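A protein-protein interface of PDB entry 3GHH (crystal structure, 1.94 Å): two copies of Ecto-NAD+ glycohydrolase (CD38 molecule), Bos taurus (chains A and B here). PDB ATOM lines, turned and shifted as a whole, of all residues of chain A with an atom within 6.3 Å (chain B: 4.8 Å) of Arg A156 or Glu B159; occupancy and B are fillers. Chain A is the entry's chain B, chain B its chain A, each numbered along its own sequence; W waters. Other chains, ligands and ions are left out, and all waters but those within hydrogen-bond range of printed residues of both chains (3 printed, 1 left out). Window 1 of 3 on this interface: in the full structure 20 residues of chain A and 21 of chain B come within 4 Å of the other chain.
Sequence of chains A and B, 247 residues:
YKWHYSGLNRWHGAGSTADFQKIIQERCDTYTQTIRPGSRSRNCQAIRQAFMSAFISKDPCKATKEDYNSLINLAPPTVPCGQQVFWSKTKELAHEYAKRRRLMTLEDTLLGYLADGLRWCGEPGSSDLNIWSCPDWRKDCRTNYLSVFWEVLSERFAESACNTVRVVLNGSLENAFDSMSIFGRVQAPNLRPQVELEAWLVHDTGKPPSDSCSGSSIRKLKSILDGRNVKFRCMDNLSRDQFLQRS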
ATOM      1  N   ILE A  72      23.747   9.433  14.403  1.00  0.00           N
ATOM      2  CA  ILE A  72      24.255   9.748  15.731  1.00  0.00           C
ATOM      3  C   ILE A  72      23.703  11.101  16.191  1.00  0.00           C
ATOM      4  O   ILE A  72      23.439  11.294  17.371  1.00  0.00           O
ATOM      5  CB  ILE A  72      25.796   9.749  15.800  1.00  0.00           C
ATOM      6  CG1 ILE A  72      26.254   9.866  17.255  1.00  0.00           C
ATOM      7  CG2 ILE A  72      26.373  10.876  14.964  1.00  0.00           C
ATOM      8  CD1 ILE A  72      27.748   9.628  17.443  1.00  0.00           C
ATOM      9  N   ASN A  73      23.504  12.027  15.258  1.00  0.00           N
ATOM     10  CA  ASN A  73      22.982  13.335  15.628  1.00  0.00           C
ATOM     11  C   ASN A  73      21.553  13.246  16.152  1.00  0.00           C
ATOM     12  O   ASN A  73      21.145  14.064  16.973  1.00  0.00           O
ATOM     13  CB  ASN A  73      23.072  14.325  14.452  1.00  0.00           C
ATOM     14  CG  ASN A  73      24.491  14.810  14.208  1.00  0.00           C
ATOM     15  OD1 ASN A  73      25.387  14.530  14.995  1.00  0.00           O
ATOM     16  ND2 ASN A  73      24.702  15.537  13.110  1.00  0.00           N
ATOM     17  N   PRO A  76      22.515  10.841  20.224  1.00  0.00           N
ATOM     18  CA  PRO A  76      23.914  10.694  20.644  1.00  0.00           C
ATOM     19  C   PRO A  76      24.025   9.782  21.862  1.00  0.00           C
ATOM     20  O   PRO A  76      23.224   9.916  22.775  1.00  0.00           O
ATOM     21  CB  PRO A  76      24.335  12.129  21.005  1.00  0.00           C
ATOM     22  CG  PRO A  76      23.319  13.019  20.351  1.00  0.00           C
ATOM     23  CD  PRO A  76      22.042  12.234  20.324  1.00  0.00           C
ATOM     24  N   PRO A  77      24.997   8.852  21.869  1.00  0.00           N
ATOM     25  CA  PRO A  77      25.089   7.888  22.980  1.00  0.00           C
ATOM     26  C   PRO A  77      25.804   8.473  24.190  1.00  0.00           C
ATOM     27  O   PRO A  77      26.899   8.038  24.545  1.00  0.00           O
ATOM     28  CB  PRO A  77      25.900   6.732  22.380  1.00  0.00           C
ATOM     29  CG  PRO A  77      26.730   7.365  21.312  1.00  0.00           C
ATOM     30  CD  PRO A  77      25.977   8.579  20.804  1.00  0.00           C
ATOM     31  N   THR A  78      25.176   9.456  24.819  1.00  0.00           N
ATOM     32  CA  THR A  78      25.775  10.137  25.956  1.00  0.00           C
ATOM     33  C   THR A  78      24.930   9.852  27.199  1.00  0.00           C
ATOM     34  O   THR A  78      23.724   9.628  27.089  1.00  0.00           O
ATOM     35  CB  THR A  78      25.883  11.658  25.700  1.00  0.00           C
ATOM     36  OG1 THR A  78      26.656  12.272  26.735  1.00  0.00           O
ATOM     37  CG2 THR A  78      24.504  12.298  25.653  1.00  0.00           C
ATOM     38  N   VAL A  79      25.571   9.831  28.367  1.00  0.00           N
ATOM     39  CA  VAL A  79      24.879   9.533  29.622  1.00  0.00           C
ATOM     40  C   VAL A  79      25.455  10.338  30.790  1.00  0.00           C
ATOM     41  O   VAL A  79      26.573  10.852  30.691  1.00  0.00           O
ATOM     42  CB  VAL A  79      24.999   8.044  29.971  1.00  0.00           C
ATOM     43  CG1 VAL A  79      24.362   7.182  28.884  1.00  0.00           C
ATOM     44  CG2 VAL A  79      26.450   7.679  30.151  1.00  0.00           C
ATOM     45  N   GLU A 151      32.365   1.460  16.114  1.00  0.00           N
ATOM     46  CA  GLU A 151      33.487   2.349  16.398  1.00  0.00           C
ATOM     47  C   GLU A 151      33.006   3.780  16.610  1.00  0.00           C
ATOM     48  O   GLU A 151      33.432   4.449  17.551  1.00  0.00           O
ATOM     49  CB  GLU A 151      34.526   2.290  15.279  1.00  0.00           C
ATOM     50  CG  GLU A 151      35.292   0.970  15.252  1.00  0.00           C
ATOM     51  CD  GLU A 151      36.176   0.833  14.023  1.00  0.00           C
ATOM     52  OE1 GLU A 151      36.257   1.806  13.238  1.00  0.00           O
ATOM     53  OE2 GLU A 151      36.778  -0.248  13.842  1.00  0.00           O
ATOM     54  N   VAL A 152      32.115   4.241  15.739  1.00  0.00           N
ATOM     55  CA  VAL A 152      31.553   5.587  15.860  1.00  0.00           C
ATOM     56  C   VAL A 152      30.829   5.769  17.198  1.00  0.00           C
ATOM     57  O   VAL A 152      31.074   6.734  17.924  1.00  0.00           O
ATOM     58  CB  VAL A 152      30.590   5.897  14.706  1.00  0.00           C
ATOM     59  CG1 VAL A 152      29.798   7.168  14.995  1.00  0.00           C
ATOM     60  CG2 VAL A 152      31.370   6.045  13.401  1.00  0.00           C
ATOM     61  N   LEU A 153      29.936   4.838  17.512  1.00  0.00           N
ATOM     62  CA  LEU A 153      29.198   4.859  18.770  1.00  0.00           C
ATOM     63  C   LEU A 153      30.153   4.801  19.954  1.00  0.00           C
ATOM     64  O   LEU A 153      30.052   5.591  20.893  1.00  0.00           O
ATOM     65  CB  LEU A 153      28.249   3.666  18.841  1.00  0.00           C
ATOM     66  CG  LEU A 153      26.914   3.959  19.525  1.00  0.00           C
ATOM     67  CD1 LEU A 153      26.181   5.038  18.733  1.00  0.00           C
ATOM     68  CD2 LEU A 153      26.061   2.700  19.663  1.00  0.00           C
ATOM     69  N   SER A 154      31.073   3.842  19.908  1.00  0.00           N
ATOM     70  CA  SER A 154      32.025   3.634  20.997  1.00  0.00           C
ATOM     71  C   SER A 154      32.831   4.890  21.285  1.00  0.00           C
ATOM     72  O   SER A 154      33.079   5.228  22.444  1.00  0.00           O
ATOM     73  CB  SER A 154      32.974   2.475  20.675  1.00  0.00           C
ATOM     74  OG  SER A 154      32.262   1.255  20.598  1.00  0.00           O
ATOM     75  N   GLU A 155      33.238   5.586  20.228  1.00  0.00           N
ATOM     76  CA  GLU A 155      34.066   6.783  20.382  1.00  0.00           C
ATOM     77  C   GLU A 155      33.331   7.900  21.121  1.00  0.00           C
ATOM     78  O   GLU A 155      33.889   8.551  22.012  1.00  0.00           O
ATOM     79  CB  GLU A 155      34.526   7.299  19.019  1.00  0.00           C
ATOM     80  CG  GLU A 155      35.166   8.674  19.083  1.00  0.00           C
ATOM     81  CD  GLU A 155      35.418   9.270  17.708  1.00  0.00           C
ATOM     82  OE1 GLU A 155      35.029   8.635  16.704  1.00  0.00           O
ATOM     83  OE2 GLU A 155      36.005  10.375  17.634  1.00  0.00           O
ATOM     84  N   ARG A 156      32.078   8.125  20.745  1.00  0.00           N
ATOM     85  CA  ARG A 156      31.301   9.213  21.337  1.00  0.00           C
ATOM     86  C   ARG A 156      30.944   8.884  22.784  1.00  0.00           C
ATOM     87  O   ARG A 156      30.924   9.759  23.648  1.00  0.00           O
ATOM     88  CB  ARG A 156      30.028   9.454  20.525  1.00  0.00           C
ATOM     89  CG  ARG A 156      29.098  10.516  21.120  1.00  0.00           C
ATOM     90  CD  ARG A 156      29.726  11.906  21.060  1.00  0.00           C
ATOM     91  NE  ARG A 156      28.696  12.938  21.126  1.00  0.00           N
ATOM     92  CZ  ARG A 156      28.022  13.379  20.070  1.00  0.00           C
ATOM     93  NH1 ARG A 156      28.287  12.893  18.862  1.00  0.00           N
ATOM     94  NH2 ARG A 156      27.091  14.313  20.218  1.00  0.00           N
ATOM     95  N   PHE A 157      30.676   7.608  23.041  1.00  0.00           N
ATOM     96  CA  PHE A 157      30.328   7.135  24.376  1.00  0.00           C
ATOM     97  C   PHE A 157      31.531   7.312  25.291  1.00  0.00           C
ATOM     98  O   PHE A 157      31.394   7.732  26.436  1.00  0.00           O
ATOM     99  CB  PHE A 157      29.907   5.664  24.285  1.00  0.00           C
ATOM    100  CG  PHE A 157      29.449   5.048  25.585  1.00  0.00           C
ATOM    101  CD1 PHE A 157      28.194   5.326  26.106  1.00  0.00           C
ATOM    102  CD2 PHE A 157      30.252   4.122  26.239  1.00  0.00           C
ATOM    103  CE1 PHE A 157      27.763   4.719  27.281  1.00  0.00           C
ATOM    104  CE2 PHE A 157      29.834   3.518  27.416  1.00  0.00           C
ATOM    105  CZ  PHE A 157      28.590   3.814  27.939  1.00  0.00           C
ATOM    106  N   ALA A 158      32.717   6.997  24.778  1.00  0.00           N
ATOM    107  CA  ALA A 158      33.948   7.174  25.543  1.00  0.00           C
ATOM    108  C   ALA A 158      34.214   8.662  25.763  1.00  0.00           C
ATOM    109  O   ALA A 158      34.595   9.087  26.854  1.00  0.00           O
ATOM    110  CB  ALA A 158      35.133   6.515  24.814  1.00  0.00           C
ATOM    111  N   GLU A 159      34.012   9.451  24.711  1.00  0.00           N
ATOM    112  CA  GLU A 159      34.195  10.892  24.791  1.00  0.00           C
ATOM    113  C   GLU A 159      33.311  11.476  25.866  1.00  0.00           C
ATOM    114  O   GLU A 159      33.684  12.441  26.538  1.00  0.00           O
ATOM    115  CB  GLU A 159      33.859  11.562  23.453  1.00  0.00           C
ATOM    116  CG  GLU A 159      34.947  11.467  22.399  1.00  0.00           C
ATOM    117  CD  GLU A 159      34.583  12.206  21.115  1.00  0.00           C
ATOM    118  OE1 GLU A 159      33.602  12.989  21.127  1.00  0.00           O
ATOM    119  OE2 GLU A 159      35.280  12.002  20.096  1.00  0.00           O
ATOM    120  N   SER A 160      32.137  10.880  26.045  1.00  0.00           N
ATOM    121  CA  SER A 160      31.120  11.489  26.888  1.00  0.00           C
ATOM    122  C   SER A 160      31.373  11.232  28.373  1.00  0.00           C
ATOM    123  O   SER A 160      30.751  11.859  29.231  1.00  0.00           O
ATOM    124  CB  SER A 160      29.720  11.000  26.477  1.00  0.00           C
ATOM    125  OG  SER A 160      29.329   9.862  27.231  1.00  0.00           O
ATOM    126  N   ALA A 161      32.298  10.325  28.679  1.00  0.00           N
ATOM    127  CA  ALA A 161      32.498   9.905  30.066  1.00  0.00           C
ATOM    128  C   ALA A 161      32.996  11.056  30.944  1.00  0.00           C
ATOM    129  O   ALA A 161      33.756  11.907  30.492  1.00  0.00           O
ATOM    130  CB  ALA A 161      33.458   8.721  30.135  1.00  0.00           C
ATOM    131  N   VAL A 186      39.752   2.359  20.554  1.00  0.00           N
ATOM    132  CA  VAL A 186      38.781   3.435  20.371  1.00  0.00           C
ATOM    133  C   VAL A 186      38.240   4.035  21.672  1.00  0.00           C
ATOM    134  O   VAL A 186      37.939   5.230  21.727  1.00  0.00           O
ATOM    135  CB  VAL A 186      37.592   2.979  19.480  1.00  0.00           C
ATOM    136  CG1 VAL A 186      36.549   4.053  19.401  1.00  0.00           C
ATOM    137  CG2 VAL A 186      38.072   2.630  18.088  1.00  0.00           C
ATOM    138  N   GLU B 155      25.442  22.850  21.035  1.00  0.00           N
ATOM    139  CA  GLU B 155      24.802  21.592  21.398  1.00  0.00           C
ATOM    140  C   GLU B 155      25.787  20.601  22.029  1.00  0.00           C
ATOM    141  O   GLU B 155      25.526  20.055  23.101  1.00  0.00           O
ATOM    142  CB  GLU B 155      24.109  20.975  20.174  1.00  0.00           C
ATOM    143  CG  GLU B 155      23.611  19.555  20.388  1.00  0.00           C
ATOM    144  CD  GLU B 155      22.877  19.001  19.171  1.00  0.00           C
ATOM    145  OE1 GLU B 155      22.391  19.801  18.341  1.00  0.00           O
ATOM    146  OE2 GLU B 155      22.792  17.763  19.046  1.00  0.00           O
ATOM    147  N   ARG B 156      26.928  20.385  21.383  1.00  0.00           N
ATOM    148  CA  ARG B 156      27.948  19.503  21.960  1.00  0.00           C
ATOM    149  C   ARG B 156      28.539  20.045  23.284  1.00  0.00           C
ATOM    150  O   ARG B 156      28.828  19.276  24.200  1.00  0.00           O
ATOM    151  CB  ARG B 156      29.073  19.245  20.950  1.00  0.00           C
ATOM    152  CG  ARG B 156      28.612  18.543  19.698  1.00  0.00           C
ATOM    153  CD  ARG B 156      28.265  17.088  19.982  1.00  0.00           C
ATOM    154  NE  ARG B 156      29.427  16.308  20.414  1.00  0.00           N
ATOM    155  CZ  ARG B 156      30.276  15.724  19.575  1.00  0.00           C
ATOM    156  NH1 ARG B 156      30.086  15.832  18.268  1.00  0.00           N
ATOM    157  NH2 ARG B 156      31.307  15.029  20.034  1.00  0.00           N
ATOM    158  N   PHE B 157      28.717  21.364  23.369  1.00  0.00           N
ATOM    159  CA  PHE B 157      29.124  22.048  24.604  1.00  0.00           C
ATOM    160  C   PHE B 157      28.151  21.697  25.748  1.00  0.00           C
ATOM    161  O   PHE B 157      28.557  21.323  26.848  1.00  0.00           O
ATOM    162  CB  PHE B 157      29.106  23.557  24.339  1.00  0.00           C
ATOM    163  CG  PHE B 157      29.670  24.415  25.444  1.00  0.00           C
ATOM    164  CD1 PHE B 157      30.996  24.325  25.819  1.00  0.00           C
ATOM    165  CD2 PHE B 157      28.880  25.393  26.036  1.00  0.00           C
ATOM    166  CE1 PHE B 157      31.516  25.163  26.804  1.00  0.00           C
ATOM    167  CE2 PHE B 157      29.389  26.225  27.016  1.00  0.00           C
ATOM    168  CZ  PHE B 157      30.707  26.115  27.401  1.00  0.00           C
ATOM    169  N   ALA B 158      26.861  21.812  25.477  1.00  0.00           N
ATOM    170  CA  ALA B 158      25.836  21.513  26.485  1.00  0.00           C
ATOM    171  C   ALA B 158      25.845  20.034  26.873  1.00  0.00           C
ATOM    172  O   ALA B 158      25.702  19.683  28.045  1.00  0.00           O
ATOM    173  CB  ALA B 158      24.445  21.937  25.975  1.00  0.00           C
ATOM    174  N   GLU B 159      26.020  19.165  25.881  1.00  0.00           N
ATOM    175  CA  GLU B 159      26.044  17.726  26.122  1.00  0.00           C
ATOM    176  C   GLU B 159      27.208  17.277  26.997  1.00  0.00           C
ATOM    177  O   GLU B 159      27.086  16.320  27.760  1.00  0.00           O
ATOM    178  CB  GLU B 159      26.070  16.958  24.793  1.00  0.00           C
ATOM    179  CG  GLU B 159      24.739  16.971  24.061  1.00  0.00           C
ATOM    180  CD  GLU B 159      24.811  16.293  22.706  1.00  0.00           C
ATOM    181  OE1 GLU B 159      25.861  15.689  22.397  1.00  0.00           O
ATOM    182  OE2 GLU B 159      23.814  16.358  21.958  1.00  0.00           O
ATOM    183  N   SER B 160      28.340  17.965  26.890  1.00  0.00           N
ATOM    184  CA  SER B 160      29.547  17.495  27.557  1.00  0.00           C
ATOM    185  C   SER B 160      29.697  18.125  28.949  1.00  0.00           C
ATOM    186  O   SER B 160      30.587  17.754  29.705  1.00  0.00           O
ATOM    187  CB  SER B 160      30.772  17.795  26.689  1.00  0.00           C
ATOM    188  OG  SER B 160      30.865  19.184  26.467  1.00  0.00           O
ATOM    189  N   ALA B 161      28.816  19.067  29.278  1.00  0.00           N
ATOM    190  CA  ALA B 161      28.856  19.767  30.563  1.00  0.00           C
ATOM    191  C   ALA B 161      28.865  18.773  31.715  1.00  0.00           C
ATOM    192  O   ALA B 161      28.244  17.719  31.634  1.00  0.00           O
ATOM    193  CB  ALA B 161      27.660  20.705  30.691  1.00  0.00           C
ATOM    194  N   ASN B 190      19.604  20.415  25.972  1.00  0.00           N
ATOM    195  CA  ASN B 190      20.575  19.359  25.684  1.00  0.00           C
ATOM    196  C   ASN B 190      21.606  19.182  26.802  1.00  0.00           C
ATOM    197  O   ASN B 190      22.520  18.366  26.697  1.00  0.00           O
ATOM    198  CB  ASN B 190      21.283  19.621  24.350  1.00  0.00           C
ATOM    199  CG  ASN B 190      20.371  19.398  23.155  1.00  0.00           C
ATOM    200  OD1 ASN B 190      20.100  20.315  22.384  1.00  0.00           O
ATOM    201  ND2 ASN B 190      19.880  18.178  23.011  1.00  0.00           N
ATOM    202  N   ARG B 192      23.594  17.949  29.781  1.00  0.00           N
ATOM    203  CA  ARG B 192      23.781  16.611  30.322  1.00  0.00           C
ATOM    204  C   ARG B 192      22.960  16.474  31.592  1.00  0.00           C
ATOM    205  O   ARG B 192      22.978  17.360  32.455  1.00  0.00           O
ATOM    206  CB  ARG B 192      25.260  16.335  30.629  1.00  0.00           C
ATOM    207  CG  ARG B 192      25.524  14.890  31.057  1.00  0.00           C
ATOM    208  CD  ARG B 192      26.846  14.723  31.770  1.00  0.00           C
ATOM    209  NE  ARG B 192      28.020  15.143  30.986  1.00  0.00           N
ATOM    210  CZ  ARG B 192      28.735  14.347  30.194  1.00  0.00           C
ATOM    211  NH1 ARG B 192      28.385  13.076  30.024  1.00  0.00           N
ATOM    212  NH2 ARG B 192      29.802  14.826  29.560  1.00  0.00           N
HETATM  213  O   HOH W   1      25.004  14.442  27.788  1.00  0.00           O
HETATM  214  O   HOH W   2      32.285  14.547  27.784  1.00  0.00           O
HETATM  215  O   HOH W   3      24.388  15.653  18.984  1.00  0.00           O
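Among the printed residues, pairs that only touch across the chains: Pro A76 with Glu B159 and Thr A78 with Arg B192.
Arg A156 touches its own counterpart, Arg B156. Arg A156 touches Glu B159, and with the chains exchanged Glu A159 touches Arg B156.
Arg A156 touches just these residues of chain B: Arg B156 (3.0 Å) and Glu B159 (2.9 Å). Of chain A, only Pro A76 (3.7 Å) and Arg A156 (2.9 Å) come within 4 Å of Glu B159. Of the printed residues of chain B, Thr A78 touches Arg B192. Of the printed residues of chain B, Glu A159 touches Arg B156. Of the printed residues of chain A, Arg B156 touches Arg A156 and Glu A159. The nearest printed residue of chain B that does not touch Arg A156 is Glu B155 (5.6 Å). The nearest residue of chain A that does not touch Glu B159 is Thr A78 (4.2 Å).
The backbone carbonyl oxygen (O) of Ser B160 sits at hydrogen-bond distance from the guanidinium group (NH2) of Arg B192, 3.0 Å away. The backbone carbonyl oxygen (O) of Ala B161 lies within hydrogen-bond range of the guanidinium group (NE) of Arg B192. The backbone carbonyl oxygen (O) of Arg B156 is in hydrogen-bond range of the side-chain hydroxyl (OG) of Ser B160, at 3.0 Å. The backbone carbonyl oxygen (O) of Phe A157 is in hydrogen-bond range of the side-chain hydroxyl (OG) of Ser A160. O of Ala B158 is in hydrogen-bond range of N of Arg B192, at 3.2 Å.
The guanidinium group (NH2) of Arg A156 is in salt-bridge range of the side-chain carboxylate (OE1) of Glu B159 (2.9 Å). The guanidinium group (NH1) of Arg B192 is in hydrogen-bond range of the backbone carbonyl oxygen (O) of Val A79, 2.9 Å away. NH2 of Arg B156 lies within salt-bridge range of OE1 of Glu A159 (3.3 Å). The backbone carbonyl oxygen of Ser A160 lies within hydrogen-bond range of the guanidinium group of Arg B192, at 2.8 Å. The guanidinium group of Arg B156 lies close to the guanidinium group of Arg A156 (3.1 Å).
Water W3 lies within hydrogen-bond range of the side-chain carboxylate (OE2) of Glu B155 (2.6 Å), the side-chain carboxylate (OE2) of Glu B159 (3.1 Å) and the guanidinium group (NH2) of Arg A156 (3.3 Å). Water W1 bridges the backbone carbonyl oxygen (O) of Glu B159 (2.8 Å) and the side-chain hydroxyl (OG1) of Thr A78 (2.9 Å). Water W2 lies within hydrogen-bond range of the backbone carbonyl oxygen of Glu A159 (2.8 Å), the guanidinium group of Arg B192 (3.1 Å) and the backbone carbonyl oxygen of Ser A160 (3.4 Å).
Along chain B the printed residues that touch a printed residue of chain A span positions 156 to 192. Printed residues of chain A that touch a printed residue of chain B: Pro A76, Thr A78, Val A79, Arg A156, Glu A159 and Ser A160. Among the printed residues, 7 pairs touch across the chains.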
